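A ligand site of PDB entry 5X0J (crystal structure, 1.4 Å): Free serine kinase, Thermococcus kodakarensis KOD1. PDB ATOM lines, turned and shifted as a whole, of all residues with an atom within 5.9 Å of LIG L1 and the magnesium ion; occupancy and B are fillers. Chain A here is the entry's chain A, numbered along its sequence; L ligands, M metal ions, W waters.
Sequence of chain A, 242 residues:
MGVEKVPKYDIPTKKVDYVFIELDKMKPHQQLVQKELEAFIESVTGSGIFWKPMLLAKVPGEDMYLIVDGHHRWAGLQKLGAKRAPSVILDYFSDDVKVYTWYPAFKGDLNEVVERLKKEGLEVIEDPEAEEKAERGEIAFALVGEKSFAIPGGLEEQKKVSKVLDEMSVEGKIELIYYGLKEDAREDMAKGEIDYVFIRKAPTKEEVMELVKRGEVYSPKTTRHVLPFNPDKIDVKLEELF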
ATOM      1  N   GLY A   2     -17.416  -3.514 -21.206  1.00  0.00           N
ATOM      2  CA  GLY A   2     -18.309  -2.889 -20.189  1.00  0.00           C
ATOM      3  C   GLY A   2     -19.761  -3.054 -20.552  1.00  0.00           C
ATOM      4  O   GLY A   2     -20.095  -3.849 -21.438  1.00  0.00           O
ATOM      5  N   GLU A   4     -21.867  -0.799 -21.892  1.00  0.00           N
ATOM      6  CA  GLU A   4     -22.409   0.011 -22.994  1.00  0.00           C
ATOM      7  C   GLU A   4     -22.243  -0.662 -24.345  1.00  0.00           C
ATOM      8  O   GLU A   4     -21.222  -1.293 -24.631  1.00  0.00           O
ATOM      9  CB  GLU A   4     -21.737   1.382 -23.028  1.00  0.00           C
ATOM     10  CG  GLU A   4     -22.080   2.253 -21.823  1.00  0.00           C
ATOM     11  CD  GLU A   4     -21.021   3.282 -21.469  1.00  0.00           C
ATOM     12  OE1 GLU A   4     -19.816   3.038 -21.694  1.00  0.00           O
ATOM     13  OE2 GLU A   4     -21.401   4.301 -20.877  1.00  0.00           O
ATOM     14  N   GLU A  36     -20.393  -2.515 -14.426  1.00  0.00           N
ATOM     15  CA  GLU A  36     -19.475  -1.570 -15.086  1.00  0.00           C
ATOM     16  C   GLU A  36     -18.272  -1.285 -14.177  1.00  0.00           C
ATOM     17  O   GLU A  36     -17.130  -1.284 -14.639  1.00  0.00           O
ATOM     18  CB  GLU A  36     -20.235  -0.279 -15.417  1.00  0.00           C
ATOM     19  CG  GLU A  36     -19.489   0.795 -16.202  1.00  0.00           C
ATOM     20  CD  GLU A  36     -19.428   0.576 -17.697  1.00  0.00           C
ATOM     21  OE1 GLU A  36     -19.666   1.552 -18.442  1.00  0.00           O
ATOM     22  OE2 GLU A  36     -19.195  -0.575 -18.117  1.00  0.00           O
ATOM     23  N   ALA A  39     -16.084  -4.533 -13.994  1.00  0.00           N
ATOM     24  CA  ALA A  39     -15.335  -4.761 -15.237  1.00  0.00           C
ATOM     25  C   ALA A  39     -14.155  -3.807 -15.359  1.00  0.00           C
ATOM     26  O   ALA A  39     -13.074  -4.227 -15.756  1.00  0.00           O
ATOM     27  CB  ALA A  39     -16.252  -4.631 -16.447  1.00  0.00           C
ATOM     28  N   PHE A  40     -14.350  -2.547 -14.993  1.00  0.00           N
ATOM     29  CA  PHE A  40     -13.229  -1.620 -14.987  1.00  0.00           C
ATOM     30  C   PHE A  40     -12.130  -2.071 -14.016  1.00  0.00           C
ATOM     31  O   PHE A  40     -10.961  -2.080 -14.366  1.00  0.00           O
ATOM     32  CB  PHE A  40     -13.638  -0.188 -14.663  1.00  0.00           C
ATOM     33  CG  PHE A  40     -12.454   0.659 -14.364  1.00  0.00           C
ATOM     34  CD1 PHE A  40     -11.564   0.989 -15.384  1.00  0.00           C
ATOM     35  CD2 PHE A  40     -12.128   1.005 -13.062  1.00  0.00           C
ATOM     36  CE1 PHE A  40     -10.403   1.709 -15.105  1.00  0.00           C
ATOM     37  CE2 PHE A  40     -10.989   1.729 -12.782  1.00  0.00           C
ATOM     38  CZ  PHE A  40     -10.122   2.086 -13.804  1.00  0.00           C
ATOM     39  N   SER A  43     -10.306  -5.134 -15.359  1.00  0.00           N
ATOM     40  CA  SER A  43      -9.519  -4.756 -16.532  1.00  0.00           C
ATOM     41  C   SER A  43      -8.242  -4.011 -16.152  1.00  0.00           C
ATOM     42  O   SER A  43      -7.177  -4.361 -16.611  1.00  0.00           O
ATOM     43  CB  SER A  43     -10.336  -3.879 -17.481  1.00  0.00           C
ATOM     44  OG  SER A  43      -9.511  -3.411 -18.537  1.00  0.00           O
ATOM     45  N   VAL A  44      -8.361  -2.980 -15.315  1.00  0.00           N
ATOM     46  CA  VAL A  44      -7.192  -2.139 -15.022  1.00  0.00           C
ATOM     47  C   VAL A  44      -6.164  -2.904 -14.168  1.00  0.00           C
ATOM     48  O   VAL A  44      -4.968  -2.804 -14.425  1.00  0.00           O
ATOM     49  CB  VAL A  44      -7.609  -0.766 -14.432  1.00  0.00           C
ATOM     50  CG1 VAL A  44      -8.001  -0.856 -12.965  1.00  0.00           C
ATOM     51  CG2 VAL A  44      -6.510   0.255 -14.630  1.00  0.00           C
ATOM     52  N   SER A  47      -4.769  -6.002 -16.513  1.00  0.00           N
ATOM     53  CA  SER A  47      -3.930  -5.544 -17.627  1.00  0.00           C
ATOM     54  C   SER A  47      -2.749  -4.698 -17.186  1.00  0.00           C
ATOM     55  O   SER A  47      -1.717  -4.700 -17.851  1.00  0.00           O
ATOM     56  CB  SER A  47      -4.769  -4.775 -18.636  1.00  0.00           C
ATOM     57  OG  SER A  47      -5.086  -3.496 -18.142  1.00  0.00           O
ATOM     58  N   ILE A  49      -2.754  -1.468 -17.270  1.00  0.00           N
ATOM     59  CA  ILE A  49      -2.730  -0.280 -18.137  1.00  0.00           C
ATOM     60  C   ILE A  49      -4.073   0.431 -18.034  1.00  0.00           C
ATOM     61  O   ILE A  49      -5.127  -0.205 -18.093  1.00  0.00           O
ATOM     62  CB  ILE A  49      -2.469  -0.641 -19.619  1.00  0.00           C
ATOM     63  CG1 ILE A  49      -1.035  -1.156 -19.797  1.00  0.00           C
ATOM     64  CG2 ILE A  49      -2.718   0.530 -20.562  1.00  0.00           C
ATOM     65  CD1 ILE A  49       0.062  -0.139 -19.560  1.00  0.00           C
ATOM     66  N   PHE A  50      -3.996   1.751 -17.871  1.00  0.00           N
ATOM     67  CA  PHE A  50      -5.155   2.647 -17.882  1.00  0.00           C
ATOM     68  C   PHE A  50      -5.092   3.368 -19.223  1.00  0.00           C
ATOM     69  O   PHE A  50      -4.183   4.144 -19.453  1.00  0.00           O
ATOM     70  CB  PHE A  50      -5.073   3.607 -16.691  1.00  0.00           C
ATOM     71  CG  PHE A  50      -6.265   4.503 -16.533  1.00  0.00           C
ATOM     72  CD1 PHE A  50      -6.367   5.686 -17.254  1.00  0.00           C
ATOM     73  CD2 PHE A  50      -7.284   4.179 -15.645  1.00  0.00           C
ATOM     74  CE1 PHE A  50      -7.457   6.516 -17.088  1.00  0.00           C
ATOM     75  CE2 PHE A  50      -8.398   5.026 -15.484  1.00  0.00           C
ATOM     76  CZ  PHE A  50      -8.450   6.189 -16.214  1.00  0.00           C
ATOM     77  N   TRP A  51      -6.040   3.078 -20.125  1.00  0.00           N
ATOM     78  CA  TRP A  51      -5.919   3.477 -21.534  1.00  0.00           C
ATOM     79  C   TRP A  51      -6.912   4.523 -22.040  1.00  0.00           C
ATOM     80  O   TRP A  51      -6.826   4.914 -23.198  1.00  0.00           O
ATOM     81  CB  TRP A  51      -5.919   2.231 -22.465  1.00  0.00           C
ATOM     82  CG  TRP A  51      -7.110   1.320 -22.288  1.00  0.00           C
ATOM     83  CD1 TRP A  51      -7.154   0.158 -21.567  1.00  0.00           C
ATOM     84  CD2 TRP A  51      -8.433   1.508 -22.809  1.00  0.00           C
ATOM     85  NE1 TRP A  51      -8.410  -0.390 -21.632  1.00  0.00           N
ATOM     86  CE2 TRP A  51      -9.222   0.417 -22.372  1.00  0.00           C
ATOM     87  CE3 TRP A  51      -9.022   2.484 -23.630  1.00  0.00           C
ATOM     88  CZ2 TRP A  51     -10.574   0.286 -22.704  1.00  0.00           C
ATOM     89  CZ3 TRP A  51     -10.381   2.346 -23.973  1.00  0.00           C
ATOM     90  CH2 TRP A  51     -11.128   1.249 -23.500  1.00  0.00           C
ATOM     91  N   LYS A  52      -7.825   4.983 -21.198  1.00  0.00           N
ATOM     92  CA  LYS A  52      -8.867   5.923 -21.608  1.00  0.00           C
ATOM     93  C   LYS A  52      -8.932   7.085 -20.613  1.00  0.00           C
ATOM     94  O   LYS A  52      -9.310   6.878 -19.475  1.00  0.00           O
ATOM     95  CB  LYS A  52     -10.236   5.230 -21.665  1.00  0.00           C
ATOM     96  CG  LYS A  52     -11.321   6.114 -22.248  1.00  0.00           C
ATOM     97  CD  LYS A  52     -12.707   5.480 -22.181  1.00  0.00           C
ATOM     98  CE  LYS A  52     -12.920   4.421 -23.220  1.00  0.00           C
ATOM     99  NZ  LYS A  52     -14.373   4.135 -23.376  1.00  0.00           N
ATOM    100  N   ASP A  69     -17.392  12.250 -18.055  1.00  0.00           N
ATOM    101  CA  ASP A  69     -17.427  10.831 -18.333  1.00  0.00           C
ATOM    102  C   ASP A  69     -16.315  10.197 -17.537  1.00  0.00           C
ATOM    103  O   ASP A  69     -15.176  10.684 -17.549  1.00  0.00           O
ATOM    104  CB  ASP A  69     -17.223  10.594 -19.837  1.00  0.00           C
ATOM    105  CG  ASP A  69     -17.233   9.117 -20.206  1.00  0.00           C
ATOM    106  OD1 ASP A  69     -17.914   8.318 -19.538  1.00  0.00           O
ATOM    107  OD2 ASP A  69     -16.537   8.769 -21.192  1.00  0.00           O
ATOM    108  N   GLY A  70     -16.646   9.129 -16.811  1.00  0.00           N
ATOM    109  CA  GLY A  70     -15.663   8.439 -15.968  1.00  0.00           C
ATOM    110  C   GLY A  70     -16.068   8.121 -14.548  1.00  0.00           C
ATOM    111  O   GLY A  70     -15.201   7.985 -13.679  1.00  0.00           O
ATOM    112  N   HIS A  71     -17.353   7.964 -14.277  1.00  0.00           N
ATOM    113  CA  HIS A  71     -17.794   7.664 -12.903  1.00  0.00           C
ATOM    114  C   HIS A  71     -17.235   6.368 -12.352  1.00  0.00           C
ATOM    115  O   HIS A  71     -16.879   6.294 -11.173  1.00  0.00           O
ATOM    116  CB  HIS A  71     -19.304   7.666 -12.837  1.00  0.00           C
ATOM    117  CG  HIS A  71     -19.878   9.028 -12.970  1.00  0.00           C
ATOM    118  ND1 HIS A  71     -20.006   9.657 -14.183  1.00  0.00           N
ATOM    119  CD2 HIS A  71     -20.250   9.935 -12.032  1.00  0.00           C
ATOM    120  CE1 HIS A  71     -20.480  10.874 -14.005  1.00  0.00           C
ATOM    121  NE2 HIS A  71     -20.618  11.060 -12.705  1.00  0.00           N
ATOM    122  N   HIS A  72     -17.149   5.359 -13.211  1.00  0.00           N
ATOM    123  CA  HIS A  72     -16.719   4.024 -12.783  1.00  0.00           C
ATOM    124  C   HIS A  72     -15.212   3.959 -12.657  1.00  0.00           C
ATOM    125  O   HIS A  72     -14.697   3.384 -11.684  1.00  0.00           O
ATOM    126  CB  HIS A  72     -17.305   2.969 -13.710  1.00  0.00           C
ATOM    127  CG  HIS A  72     -18.805   2.972 -13.708  1.00  0.00           C
ATOM    128  ND1 HIS A  72     -19.546   3.878 -14.439  1.00  0.00           N
ATOM    129  CD2 HIS A  72     -19.691   2.231 -13.007  1.00  0.00           C
ATOM    130  CE1 HIS A  72     -20.829   3.657 -14.214  1.00  0.00           C
ATOM    131  NE2 HIS A  72     -20.936   2.670 -13.366  1.00  0.00           N
ATOM    132  N   ARG A  73     -14.508   4.565 -13.604  1.00  0.00           N
ATOM    133  CA  ARG A  73     -13.060   4.717 -13.455  1.00  0.00           C
ATOM    134  C   ARG A  73     -12.736   5.448 -12.138  1.00  0.00           C
ATOM    135  O   ARG A  73     -11.849   5.015 -11.368  1.00  0.00           O
ATOM    136  CB  ARG A  73     -12.445   5.457 -14.628  1.00  0.00           C
ATOM    137  CG  ARG A  73     -12.187   4.575 -15.839  1.00  0.00           C
ATOM    138  CD  ARG A  73     -11.970   5.380 -17.101  1.00  0.00           C
ATOM    139  NE  ARG A  73     -13.224   5.937 -17.603  1.00  0.00           N
ATOM    140  CZ  ARG A  73     -13.326   6.850 -18.568  1.00  0.00           C
ATOM    141  NH1 ARG A  73     -12.234   7.327 -19.183  1.00  0.00           N
ATOM    142  NH2 ARG A  73     -14.523   7.264 -18.960  1.00  0.00           N
ATOM    143  N   TRP A  74     -13.443   6.541 -11.882  1.00  0.00           N
ATOM    144  CA  TRP A  74     -13.187   7.339 -10.659  1.00  0.00           C
ATOM    145  C   TRP A  74     -13.461   6.525  -9.394  1.00  0.00           C
ATOM    146  O   TRP A  74     -12.608   6.431  -8.515  1.00  0.00           O
ATOM    147  CB  TRP A  74     -14.040   8.616 -10.700  1.00  0.00           C
ATOM    148  CG  TRP A  74     -14.113   9.402  -9.428  1.00  0.00           C
ATOM    149  CD1 TRP A  74     -13.176  10.270  -8.936  1.00  0.00           C
ATOM    150  CD2 TRP A  74     -15.206   9.421  -8.503  1.00  0.00           C
ATOM    151  NE1 TRP A  74     -13.623  10.824  -7.762  1.00  0.00           N
ATOM    152  CE2 TRP A  74     -14.864  10.329  -7.476  1.00  0.00           C
ATOM    153  CE3 TRP A  74     -16.454   8.771  -8.454  1.00  0.00           C
ATOM    154  CZ2 TRP A  74     -15.727  10.573  -6.380  1.00  0.00           C
ATOM    155  CZ3 TRP A  74     -17.308   9.019  -7.385  1.00  0.00           C
ATOM    156  CH2 TRP A  74     -16.932   9.919  -6.355  1.00  0.00           C
ATOM    157  N   TRP A 102     -28.110   7.522 -22.255  1.00  0.00           N
ATOM    158  CA  TRP A 102     -27.963   6.098 -22.452  1.00  0.00           C
ATOM    159  C   TRP A 102     -29.277   5.460 -22.024  1.00  0.00           C
ATOM    160  O   TRP A 102     -29.833   5.804 -20.971  1.00  0.00           O
ATOM    161  CB  TRP A 102     -26.848   5.512 -21.595  1.00  0.00           C
ATOM    162  CG  TRP A 102     -25.482   6.000 -21.924  1.00  0.00           C
ATOM    163  CD1 TRP A 102     -24.795   6.998 -21.304  1.00  0.00           C
ATOM    164  CD2 TRP A 102     -24.608   5.481 -22.931  1.00  0.00           C
ATOM    165  NE1 TRP A 102     -23.554   7.147 -21.862  1.00  0.00           N
ATOM    166  CE2 TRP A 102     -23.419   6.236 -22.878  1.00  0.00           C
ATOM    167  CE3 TRP A 102     -24.721   4.463 -23.878  1.00  0.00           C
ATOM    168  CZ2 TRP A 102     -22.342   5.995 -23.730  1.00  0.00           C
ATOM    169  CZ3 TRP A 102     -23.662   4.228 -24.743  1.00  0.00           C
ATOM    170  CH2 TRP A 102     -22.482   5.001 -24.667  1.00  0.00           C
ATOM    171  N   LYS A 221     -25.810   6.481 -15.882  1.00  0.00           N
ATOM    172  CA  LYS A 221     -25.746   6.640 -17.332  1.00  0.00           C
ATOM    173  C   LYS A 221     -26.767   7.633 -17.900  1.00  0.00           C
ATOM    174  O   LYS A 221     -27.161   7.563 -19.061  1.00  0.00           O
ATOM    175  CB  LYS A 221     -25.873   5.271 -18.016  1.00  0.00           C
ATOM    176  CG  LYS A 221     -24.859   4.231 -17.555  1.00  0.00           C
ATOM    177  CD  LYS A 221     -23.447   4.625 -17.929  1.00  0.00           C
ATOM    178  CE  LYS A 221     -22.492   3.479 -17.685  1.00  0.00           C
ATOM    179  NZ  LYS A 221     -21.093   3.821 -18.093  1.00  0.00           N
HETATM  180  P1  LIG L   1     -16.801   5.107 -16.820  1.00  0.00           P
HETATM  181  O1  LIG L   1     -15.443   5.139 -16.148  1.00  0.00           O
HETATM  182  O2  LIG L   1     -17.935   5.441 -15.859  1.00  0.00           O
HETATM  183  O3  LIG L   1     -16.810   5.903 -18.097  1.00  0.00           O
HETATM  184  O4  LIG L   1     -17.074   3.580 -17.222  1.00  0.00           O
HETATM  185  C1  LIG L   1     -16.037   2.613 -17.337  1.00  0.00           C
HETATM  186  C2  LIG L   1     -15.091   2.994 -18.450  1.00  0.00           C
HETATM  187  O5  LIG L   1     -13.849   2.340 -18.246  1.00  0.00           O
HETATM  188  C3  LIG L   1     -15.483   2.556 -19.879  1.00  0.00           C
HETATM  189  O6  LIG L   1     -15.408   3.681 -20.747  1.00  0.00           O
HETATM  190  C4  LIG L   1     -14.457   1.511 -20.332  1.00  0.00           C
HETATM  191  O7  LIG L   1     -14.180   1.558 -21.731  1.00  0.00           O
HETATM  192  C5  LIG L   1     -13.308   1.969 -19.489  1.00  0.00           C
HETATM  193  N1  LIG L   1     -12.207   1.026 -19.263  1.00  0.00           N
HETATM  194  C6  LIG L   1     -12.244  -0.323 -19.245  1.00  0.00           C
HETATM  195  N2  LIG L   1     -11.016  -0.844 -18.965  1.00  0.00           N
HETATM  196  C7  LIG L   1     -10.195   0.206 -18.797  1.00  0.00           C
HETATM  197  C8  LIG L   1      -8.763   0.379 -18.492  1.00  0.00           C
HETATM  198  N3  LIG L   1      -7.973  -0.707 -18.307  1.00  0.00           N
HETATM  199  N4  LIG L   1      -8.299   1.642 -18.408  1.00  0.00           N
HETATM  200  C9  LIG L   1      -9.074   2.734 -18.587  1.00  0.00           C
HETATM  201  N5  LIG L   1     -10.387   2.647 -18.877  1.00  0.00           N
HETATM  202  C10 LIG L   1     -10.976   1.428 -18.988  1.00  0.00           C
HETATM  203  N1  LG2 L   2     -21.379  10.481 -18.192  1.00  0.00           N
HETATM  204  C1  LG2 L   2     -21.005   9.360 -19.110  1.00  0.00           C
HETATM  205  C2  LG2 L   2     -21.890   8.153 -18.804  1.00  0.00           C
HETATM  206  O1  LG2 L   2     -21.718   7.782 -17.431  1.00  0.00           O
HETATM  207  C3  LG2 L   2     -21.101   9.802 -20.545  1.00  0.00           C
HETATM  208  O2  LG2 L   2     -21.155   8.950 -21.455  1.00  0.00           O
HETATM  209  O3  LG2 L   2     -21.111  11.012 -20.833  1.00  0.00           O
HETATM  210  P1  LG2 L   2     -20.330   7.119 -16.917  1.00  0.00           P
HETATM  211  O4  LG2 L   2     -19.755   6.396 -18.121  1.00  0.00           O
HETATM  212  O5  LG2 L   2     -20.810   6.211 -15.824  1.00  0.00           O
HETATM  213  O6  LG2 L   2     -19.500   8.282 -16.421  1.00  0.00           O
HETATM  214 MG    MG M   1     -18.304   6.267 -19.458  1.00  0.00          MG
HETATM  215  O   HOH W   1     -18.460   4.153 -19.651  1.00  0.00           O
HETATM  216  O   HOH W   2     -16.890   6.064 -21.037  1.00  0.00           O
HETATM  217  O   HOH W   3     -14.503  -0.932 -22.412  1.00  0.00           O
HETATM  218  O   HOH W   4     -19.740   6.458 -21.038  1.00  0.00           O
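O2 of LIG L1 is in hydrogen-bond range of N of His 72 (2.8 Å).
A ring nitrogen (ND1) of His 72 lies within hydrogen-bond range of an oxygen (O2) of LIG L1, 2.7 Å away.
The backbone NH (N) of Arg 73 lies within hydrogen-bond range of an oxygen (O1) of LIG L1.
The guanidinium group (NE) of Arg 73 is in salt-bridge range of an oxygen (O1) of LIG L1, at 2.8 Å.
The side-chain amino group of Lys 52 lies within hydrogen-bond range of an oxygen (O6) of LIG L1.
N3 of LIG L1 is in hydrogen-bond range of O of Ile 49 (2.9 Å).
OG of Ser 43 is in hydrogen-bond range of N2 of LIG L1, 3.0 Å away.
O2 of LIG L1 sits at hydrogen-bond distance from N of His 71 (3.0 Å).
The backbone NH of Trp 51 is in hydrogen-bond range of a nitrogen (N4) of LIG L1 (3.2 Å).
An oxygen (O3) of LIG L1 sits close to the backbone NH (N) of Gly 70, at 3.5 Å.
A ring nitrogen (ND1) of His 72 lies within hydrogen-bond range of an oxygen (O5) of LG2 L2, at 3.0 Å.
The backbone NH (N) of His 71 lies within hydrogen-bond range of an oxygen (O6) of LG2 L2.
A ring nitrogen (ND1) of His 71 is in hydrogen-bond range of an oxygen (O6) of LG2 L2 (2.7 Å).
N of Gly 70 sits at hydrogen-bond distance from O6 of LG2 L2.
NZ of Lys 221 lies within salt-bridge range of O5 of LG2 L2, 3.3 Å away.
An oxygen (O2) of LG2 L2 is in hydrogen-bond range of the indole nitrogen (NE1) of Trp 102 (3.0 Å).
OD2 of Asp 69 lies within salt-bridge range of NH2 of Arg 73, at 3.4 Å.
The guanidinium group of Arg 73 sits at hydrogen-bond distance from the backbone carbonyl oxygen of Lys 52 (3.0 Å).
The backbone NH (N) of Ile 49 sits at hydrogen-bond distance from the side-chain hydroxyl (OG) of Ser 47 (3.2 Å).
O of Ser 43 sits at hydrogen-bond distance from OG of Ser 47 (2.7 Å).
The side-chain carboxylate (OE1) of Glu 36 lies within salt-bridge range of the side-chain amino group (NZ) of Lys 221.
NZ of Lys 221 lies within salt-bridge range of OE2 of Glu 4 (2.8 Å).
N of Trp 102 lies close to O of Lys 221, 3.3 Å away.
Glu 36 touches LIG L1.
Phe 40 touches LIG L1 (CD1 to C10, 3.7 Å).
Val 44 touches LIG L1 (CA to N3, 3.7 Å).
Phe 50 touches LIG L1 (CA to N4, 3.3 Å).
Hydrophobic or aromatic side chains within 4 Å of LIG L1: Phe 40, Val 44, Phe 50, Trp 51, His 71 and His 72.
The nearest printed residue that does not touch LIG L1 is Ser 47 (4.02 Å).
Residues that only touch the magnesium ion: Glu 4, Arg 73 and Lys 221.
Of the 20 residues printed, 4 come within 4 Å of the magnesium ion.
The magnesium ion is bound by O4 of LG2 L2 (2.0 Å), O3 of LIG L1 (2.1 Å), OD1 of Asp 69 (2.1 Å), water W1 (2.1 Å), water W2 (2.1 Å) and water W4 (2.1 Å).
The magnesium ion has six donor atoms within binding distance.
Water W2 lies within hydrogen-bond range of OD2 of Asp 69 (2.7 Å), O6 of LIG L1 (2.8 Å) and NH2 of Arg 73 (3.4 Å).
Water W4 lies within hydrogen-bond range of the side-chain carboxylate of Glu 4 (2.7 Å) and an oxygen (O2) of LG2 L2 (2.9 Å).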
